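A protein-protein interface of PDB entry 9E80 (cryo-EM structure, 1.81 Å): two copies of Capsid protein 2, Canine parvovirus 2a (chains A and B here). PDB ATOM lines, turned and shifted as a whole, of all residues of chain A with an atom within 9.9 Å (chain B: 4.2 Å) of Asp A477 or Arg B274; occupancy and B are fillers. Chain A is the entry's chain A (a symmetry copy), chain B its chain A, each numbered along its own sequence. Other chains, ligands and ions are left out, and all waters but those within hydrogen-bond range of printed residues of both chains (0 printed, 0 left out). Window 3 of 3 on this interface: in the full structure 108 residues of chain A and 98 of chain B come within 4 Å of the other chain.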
ATOM      1  N   GLU A 473     -22.485  12.662  21.229  1.00  0.00           N
ATOM      2  CA  GLU A 473     -23.576  12.042  20.491  1.00  0.00           C
ATOM      3  C   GLU A 473     -24.254  10.972  21.340  1.00  0.00           C
ATOM      4  O   GLU A 473     -23.610  10.283  22.136  1.00  0.00           O
ATOM      5  CB  GLU A 473     -23.060  11.428  19.190  1.00  0.00           C
ATOM      6  CG  GLU A 473     -24.137  10.804  18.328  1.00  0.00           C
ATOM      7  CD  GLU A 473     -25.188  11.804  17.891  1.00  0.00           C
ATOM      8  OE1 GLU A 473     -26.081  12.121  18.701  1.00  0.00           O
ATOM      9  OE2 GLU A 473     -25.117  12.272  16.735  1.00  0.00           O
ATOM     10  N   PHE A 474     -25.563  10.834  21.158  1.00  0.00           N
ATOM     11  CA  PHE A 474     -26.332   9.859  21.916  1.00  0.00           C
ATOM     12  C   PHE A 474     -25.911   8.441  21.549  1.00  0.00           C
ATOM     13  O   PHE A 474     -25.477   8.168  20.428  1.00  0.00           O
ATOM     14  CB  PHE A 474     -27.829  10.028  21.648  1.00  0.00           C
ATOM     15  CG  PHE A 474     -28.419  11.294  22.209  1.00  0.00           C
ATOM     16  CD1 PHE A 474     -27.630  12.226  22.866  1.00  0.00           C
ATOM     17  CD2 PHE A 474     -29.773  11.550  22.074  1.00  0.00           C
ATOM     18  CE1 PHE A 474     -28.181  13.384  23.373  1.00  0.00           C
ATOM     19  CE2 PHE A 474     -30.329  12.705  22.582  1.00  0.00           C
ATOM     20  CZ  PHE A 474     -29.531  13.624  23.231  1.00  0.00           C
ATOM     21  N   ASP A 475     -26.058   7.528  22.507  1.00  0.00           N
ATOM     22  CA  ASP A 475     -25.750   6.117  22.284  1.00  0.00           C
ATOM     23  C   ASP A 475     -26.994   5.325  21.915  1.00  0.00           C
ATOM     24  O   ASP A 475     -27.117   4.141  22.239  1.00  0.00           O
ATOM     25  CB  ASP A 475     -25.075   5.528  23.517  1.00  0.00           C
ATOM     26  CG  ASP A 475     -24.468   4.162  23.252  1.00  0.00           C
ATOM     27  OD1 ASP A 475     -24.311   3.803  22.065  1.00  0.00           O
ATOM     28  OD2 ASP A 475     -24.144   3.450  24.222  1.00  0.00           O
ATOM     29  N   THR A 476     -27.942   5.972  21.244  1.00  0.00           N
ATOM     30  CA  THR A 476     -29.091   5.286  20.681  1.00  0.00           C
ATOM     31  C   THR A 476     -28.717   4.654  19.344  1.00  0.00           C
ATOM     32  O   THR A 476     -27.744   5.044  18.693  1.00  0.00           O
ATOM     33  CB  THR A 476     -30.257   6.256  20.486  1.00  0.00           C
ATOM     34  OG1 THR A 476     -29.838   7.344  19.653  1.00  0.00           O
ATOM     35  CG2 THR A 476     -30.737   6.802  21.825  1.00  0.00           C
ATOM     36  N   ASP A 477     -29.509   3.662  18.934  1.00  0.00           N
ATOM     37  CA  ASP A 477     -29.270   3.026  17.643  1.00  0.00           C
ATOM     38  C   ASP A 477     -29.463   4.013  16.498  1.00  0.00           C
ATOM     39  O   ASP A 477     -28.665   4.040  15.554  1.00  0.00           O
ATOM     40  CB  ASP A 477     -30.197   1.821  17.470  1.00  0.00           C
ATOM     41  CG  ASP A 477     -30.145   0.872  18.652  1.00  0.00           C
ATOM     42  OD1 ASP A 477     -29.068   0.751  19.271  1.00  0.00           O
ATOM     43  OD2 ASP A 477     -31.181   0.246  18.960  1.00  0.00           O
ATOM     44  N   LEU A 478     -30.511   4.829  16.562  1.00  0.00           N
ATOM     45  CA  LEU A 478     -30.790   5.849  15.561  1.00  0.00           C
ATOM     46  C   LEU A 478     -30.487   7.213  16.166  1.00  0.00           C
ATOM     47  O   LEU A 478     -31.051   7.573  17.203  1.00  0.00           O
ATOM     48  CB  LEU A 478     -32.243   5.772  15.092  1.00  0.00           C
ATOM     49  CG  LEU A 478     -32.656   4.424  14.493  1.00  0.00           C
ATOM     50  CD1 LEU A 478     -34.090   4.485  13.995  1.00  0.00           C
ATOM     51  CD2 LEU A 478     -31.712   4.009  13.374  1.00  0.00           C
ATOM     52  N   LYS A 479     -29.608   7.966  15.510  1.00  0.00           N
ATOM     53  CA  LYS A 479     -29.082   9.174  16.126  1.00  0.00           C
ATOM     54  C   LYS A 479     -29.706  10.417  15.506  1.00  0.00           C
ATOM     55  O   LYS A 479     -30.069  10.408  14.325  1.00  0.00           O
ATOM     56  CB  LYS A 479     -27.563   9.230  15.960  1.00  0.00           C
ATOM     57  CG  LYS A 479     -26.867   7.931  16.352  1.00  0.00           C
ATOM     58  CD  LYS A 479     -25.588   8.190  17.117  1.00  0.00           C
ATOM     59  CE  LYS A 479     -24.821   6.905  17.415  1.00  0.00           C
ATOM     60  NZ  LYS A 479     -25.684   5.692  17.392  1.00  0.00           N
ATOM     61  N   PRO A 480     -29.845  11.503  16.268  1.00  0.00           N
ATOM     62  CA  PRO A 480     -30.409  12.731  15.699  1.00  0.00           C
ATOM     63  C   PRO A 480     -29.494  13.314  14.632  1.00  0.00           C
ATOM     64  O   PRO A 480     -28.280  13.103  14.629  1.00  0.00           O
ATOM     65  CB  PRO A 480     -30.527  13.667  16.908  1.00  0.00           C
ATOM     66  CG  PRO A 480     -29.549  13.147  17.897  1.00  0.00           C
ATOM     67  CD  PRO A 480     -29.480  11.666  17.685  1.00  0.00           C
ATOM     68  N   SER B 134     -23.600  -7.876  25.946  1.00  0.00           N
ATOM     69  CA  SER B 134     -24.039  -6.496  25.785  1.00  0.00           C
ATOM     70  C   SER B 134     -24.496  -6.171  24.371  1.00  0.00           C
ATOM     71  O   SER B 134     -25.314  -5.262  24.196  1.00  0.00           O
ATOM     72  CB  SER B 134     -22.914  -5.529  26.174  1.00  0.00           C
ATOM     73  OG  SER B 134     -21.831  -5.610  25.265  1.00  0.00           O
ATOM     74  N   PRO B 272     -24.964  -4.365  14.412  1.00  0.00           N
ATOM     75  CA  PRO B 272     -25.068  -5.069  15.694  1.00  0.00           C
ATOM     76  C   PRO B 272     -26.379  -4.752  16.395  1.00  0.00           C
ATOM     77  O   PRO B 272     -26.978  -3.693  16.199  1.00  0.00           O
ATOM     78  CB  PRO B 272     -23.870  -4.541  16.491  1.00  0.00           C
ATOM     79  CG  PRO B 272     -23.538  -3.232  15.864  1.00  0.00           C
ATOM     80  CD  PRO B 272     -23.881  -3.368  14.413  1.00  0.00           C
ATOM     81  N   CYS B 273     -26.823  -5.696  17.218  1.00  0.00           N
ATOM     82  CA  CYS B 273     -28.043  -5.551  17.999  1.00  0.00           C
ATOM     83  C   CYS B 273     -27.670  -5.394  19.468  1.00  0.00           C
ATOM     84  O   CYS B 273     -26.990  -6.257  20.035  1.00  0.00           O
ATOM     85  CB  CYS B 273     -28.959  -6.757  17.799  1.00  0.00           C
ATOM     86  SG  CYS B 273     -30.337  -6.836  18.953  1.00  0.00           S
ATOM     87  N   ARG B 274     -28.115  -4.299  20.078  1.00  0.00           N
ATOM     88  CA  ARG B 274     -27.806  -4.032  21.475  1.00  0.00           C
ATOM     89  C   ARG B 274     -28.643  -4.918  22.388  1.00  0.00           C
ATOM     90  O   ARG B 274     -29.835  -5.130  22.153  1.00  0.00           O
ATOM     91  CB  ARG B 274     -28.065  -2.562  21.812  1.00  0.00           C
ATOM     92  CG  ARG B 274     -27.318  -1.549  20.944  1.00  0.00           C
ATOM     93  CD  ARG B 274     -25.805  -1.728  20.990  1.00  0.00           C
ATOM     94  NE  ARG B 274     -25.210  -1.101  22.165  1.00  0.00           N
ATOM     95  CZ  ARG B 274     -25.002   0.201  22.299  1.00  0.00           C
ATOM     96  NH1 ARG B 274     -25.359   1.061  21.357  1.00  0.00           N
ATOM     97  NH2 ARG B 274     -24.422   0.655  23.406  1.00  0.00           N
ATOM     98  N   LEU B 275     -28.005  -5.435  23.439  1.00  0.00           N
ATOM     99  CA  LEU B 275     -28.691  -6.174  24.490  1.00  0.00           C
ATOM    100  C   LEU B 275     -28.791  -5.360  25.776  1.00  0.00           C
ATOM    101  O   LEU B 275     -28.914  -5.930  26.864  1.00  0.00           O
ATOM    102  CB  LEU B 275     -27.988  -7.508  24.749  1.00  0.00           C
ATOM    103  CG  LEU B 275     -28.018  -8.487  23.571  1.00  0.00           C
ATOM    104  CD1 LEU B 275     -27.243  -9.755  23.894  1.00  0.00           C
ATOM    105  CD2 LEU B 275     -29.450  -8.818  23.176  1.00  0.00           C
ATOM    106  N   THR B 276     -28.727  -4.038  25.664  1.00  0.00           N
ATOM    107  CA  THR B 276     -28.969  -3.125  26.768  1.00  0.00           C
ATOM    108  C   THR B 276     -30.116  -2.198  26.391  1.00  0.00           C
ATOM    109  O   THR B 276     -30.420  -2.015  25.209  1.00  0.00           O
ATOM    110  CB  THR B 276     -27.715  -2.300  27.104  1.00  0.00           C
ATOM    111  OG1 THR B 276     -27.294  -1.569  25.945  1.00  0.00           O
ATOM    112  CG2 THR B 276     -26.582  -3.205  27.567  1.00  0.00           C
ATOM    113  N   LEU B 457     -33.758   7.403  18.614  1.00  0.00           N
ATOM    114  CA  LEU B 457     -34.518   6.217  18.977  1.00  0.00           C
ATOM    115  C   LEU B 457     -33.639   4.986  18.825  1.00  0.00           C
ATOM    116  O   LEU B 457     -32.564   5.032  18.222  1.00  0.00           O
ATOM    117  CB  LEU B 457     -35.789   6.084  18.127  1.00  0.00           C
ATOM    118  CG  LEU B 457     -35.601   5.843  16.628  1.00  0.00           C
ATOM    119  CD1 LEU B 457     -36.800   5.098  16.056  1.00  0.00           C
ATOM    120  CD2 LEU B 457     -35.390   7.159  15.896  1.00  0.00           C
ATOM    121  N   ASN B 458     -34.117   3.879  19.379  1.00  0.00           N
ATOM    122  CA  ASN B 458     -33.398   2.616  19.375  1.00  0.00           C
ATOM    123  C   ASN B 458     -34.061   1.624  18.429  1.00  0.00           C
ATOM    124  O   ASN B 458     -35.218   1.783  18.029  1.00  0.00           O
ATOM    125  CB  ASN B 458     -33.344   2.026  20.785  1.00  0.00           C
ATOM    126  CG  ASN B 458     -32.457   2.823  21.715  1.00  0.00           C
ATOM    127  OD1 ASN B 458     -31.368   3.248  21.338  1.00  0.00           O
ATOM    128  ND2 ASN B 458     -32.921   3.030  22.940  1.00  0.00           N
ATOM    129  N   ASN B 459     -33.302   0.594  18.070  1.00  0.00           N
ATOM    130  CA  ASN B 459     -33.847  -0.511  17.301  1.00  0.00           C
ATOM    131  C   ASN B 459     -34.744  -1.373  18.185  1.00  0.00           C
ATOM    132  O   ASN B 459     -34.642  -1.366  19.415  1.00  0.00           O
ATOM    133  CB  ASN B 459     -32.716  -1.353  16.709  1.00  0.00           C
ATOM    134  CG  ASN B 459     -33.163  -2.179  15.518  1.00  0.00           C
ATOM    135  OD1 ASN B 459     -34.275  -2.019  15.017  1.00  0.00           O
ATOM    136  ND2 ASN B 459     -32.294  -3.072  15.060  1.00  0.00           N
ATOM    137  N   GLN B 577     -33.262  -6.995  26.718  1.00  0.00           N
ATOM    138  CA  GLN B 577     -32.442  -5.805  26.910  1.00  0.00           C
ATOM    139  C   GLN B 577     -32.385  -5.466  28.395  1.00  0.00           C
ATOM    140  O   GLN B 577     -32.594  -4.317  28.794  1.00  0.00           O
ATOM    141  CB  GLN B 577     -32.991  -4.643  26.079  1.00  0.00           C
ATOM    142  CG  GLN B 577     -32.714  -4.810  24.588  1.00  0.00           C
ATOM    143  CD  GLN B 577     -32.947  -3.542  23.786  1.00  0.00           C
ATOM    144  OE1 GLN B 577     -33.639  -2.628  24.230  1.00  0.00           O
ATOM    145  NE2 GLN B 577     -32.367  -3.486  22.592  1.00  0.00           N
ATOM    146  N   ARG B 581     -28.041   0.953  29.913  1.00  0.00           N
ATOM    147  CA  ARG B 581     -26.879   1.678  29.424  1.00  0.00           C
ATOM    148  C   ARG B 581     -27.206   3.164  29.400  1.00  0.00           C
ATOM    149  O   ARG B 581     -28.359   3.555  29.204  1.00  0.00           O
ATOM    150  CB  ARG B 581     -26.442   1.198  28.025  1.00  0.00           C
ATOM    151  CG  ARG B 581     -27.294   1.698  26.859  1.00  0.00           C
ATOM    152  CD  ARG B 581     -26.559   1.531  25.540  1.00  0.00           C
ATOM    153  NE  ARG B 581     -27.343   2.015  24.410  1.00  0.00           N
ATOM    154  CZ  ARG B 581     -28.390   1.383  23.897  1.00  0.00           C
ATOM    155  NH1 ARG B 581     -28.808   0.227  24.386  1.00  0.00           N
ATOM    156  NH2 ARG B 581     -29.032   1.925  22.866  1.00  0.00           N
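Of the printed residues of chain B, Asp A475 touches Arg B274 (2.9 Å) and Arg B581 (3.0 Å). Of the printed residues of chain B, Thr A476 touches Leu B457 (3.5 Å) and Asn B458 (3.1 Å). Of chain B, only Arg B274 (3.3 Å), Leu B457 (3.4 Å), Asn B458 (3.1 Å), Asn B459 (2.3 Å) and Arg B581 (3.8 Å) come within 4 Å of Asp A477. Of the printed residues of chain B, Leu A478 touches Leu B457 (2.6 Å). No residue of chain A comes within 4 Å of Cys B273. Of chain A, only Asp A475 (2.9 Å) and Asp A477 (3.3 Å) come within 4 Å of Arg B274. No residue of chain A comes within 4 Å of Leu B275. No residue of chain A comes within 4 Å of Thr B276. Of the printed residues of chain A, Leu B457 touches Thr A476, Asp A477 and Leu A478. Asn B458 touches just these residues of chain A: Thr A476 (3.1 Å) and Asp A477 (3.1 Å). Printed residues of chain A within 4 Å of Arg B581: Asp A475 and Asp A477. The nearest printed residue of chain B that does not touch Asp A477 is Gln B577 (5.3 Å). The nearest residue of chain A that does not touch Arg B274 is Thr A476 (5.3 Å). The nearest printed residue of chain B that does not touch Thr A476 is Arg B581 (4.01 Å).
Of the 11 printed residues of chain B, 5 touch a printed residue of chain A. Of the 8 printed residues of chain A, 4 touch a printed residue of chain B. Hydrophobic or aromatic side chains of chain A within 4 Å of the printed part of chain B: Leu A478. Among the printed residues, Asp or Glu carboxylates within 4 Å of a Lys or Arg side-chain nitrogen of the other chain: Asp A475 with Arg B274, Asp A475 with Arg B581 and Asp A477 with Arg B581.
The side-chain amide nitrogen of Gln B577 is in hydrogen-bond range of the backbone carbonyl oxygen of Arg B274 (3.1 Å). OG1 of Thr B276 is in hydrogen-bond range of NH1 of Arg B581 (2.8 Å). OD1 of Asn B458 sits at hydrogen-bond distance from NH2 of Arg B581 (3.1 Å). The side-chain hydroxyl (OG1) of Thr A476 is in hydrogen-bond range of the backbone carbonyl oxygen (O) of Leu A478 (2.7 Å). The side-chain amino group (NZ) of Lys A479 sits at hydrogen-bond distance from the backbone carbonyl oxygen (O) of Thr A476, 2.5 Å away.
Among the printed residues, merely in contact across the chains: Thr A476 with Asn B458, Asp A477 with Arg B274 and Thr A476 with Leu B457.
The guanidinium group (NH2) of Arg B274 lies within salt-bridge range of the side-chain carboxylate (OD2) of Asp A475 (2.9 Å). The backbone carbonyl oxygen (O) of Leu B457 lies within hydrogen-bond range of the backbone NH (N) of Asp A477 (3.4 Å). N of Leu A478 is in hydrogen-bond range of O of Leu B457 (2.6 Å). OD1 of Asn B458 sits at hydrogen-bond distance from N of Asp A477, at 3.1 Å. OD2 of Asp A475 lies within salt-bridge range of NE of Arg B581, at 3.5 Å. The side-chain carboxylate (OD1) of Asp A477 is in salt-bridge range of the guanidinium group (NH2) of Arg B581, at 3.8 Å. The backbone NH of Asn B459 lies close to the side-chain carboxylate of Asp A477 (2.3 Å).
No position is printed for both chains. Of the 10 pairs that touch across the chains among the printed residues, none has its exchanged pair printed and touching as well.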
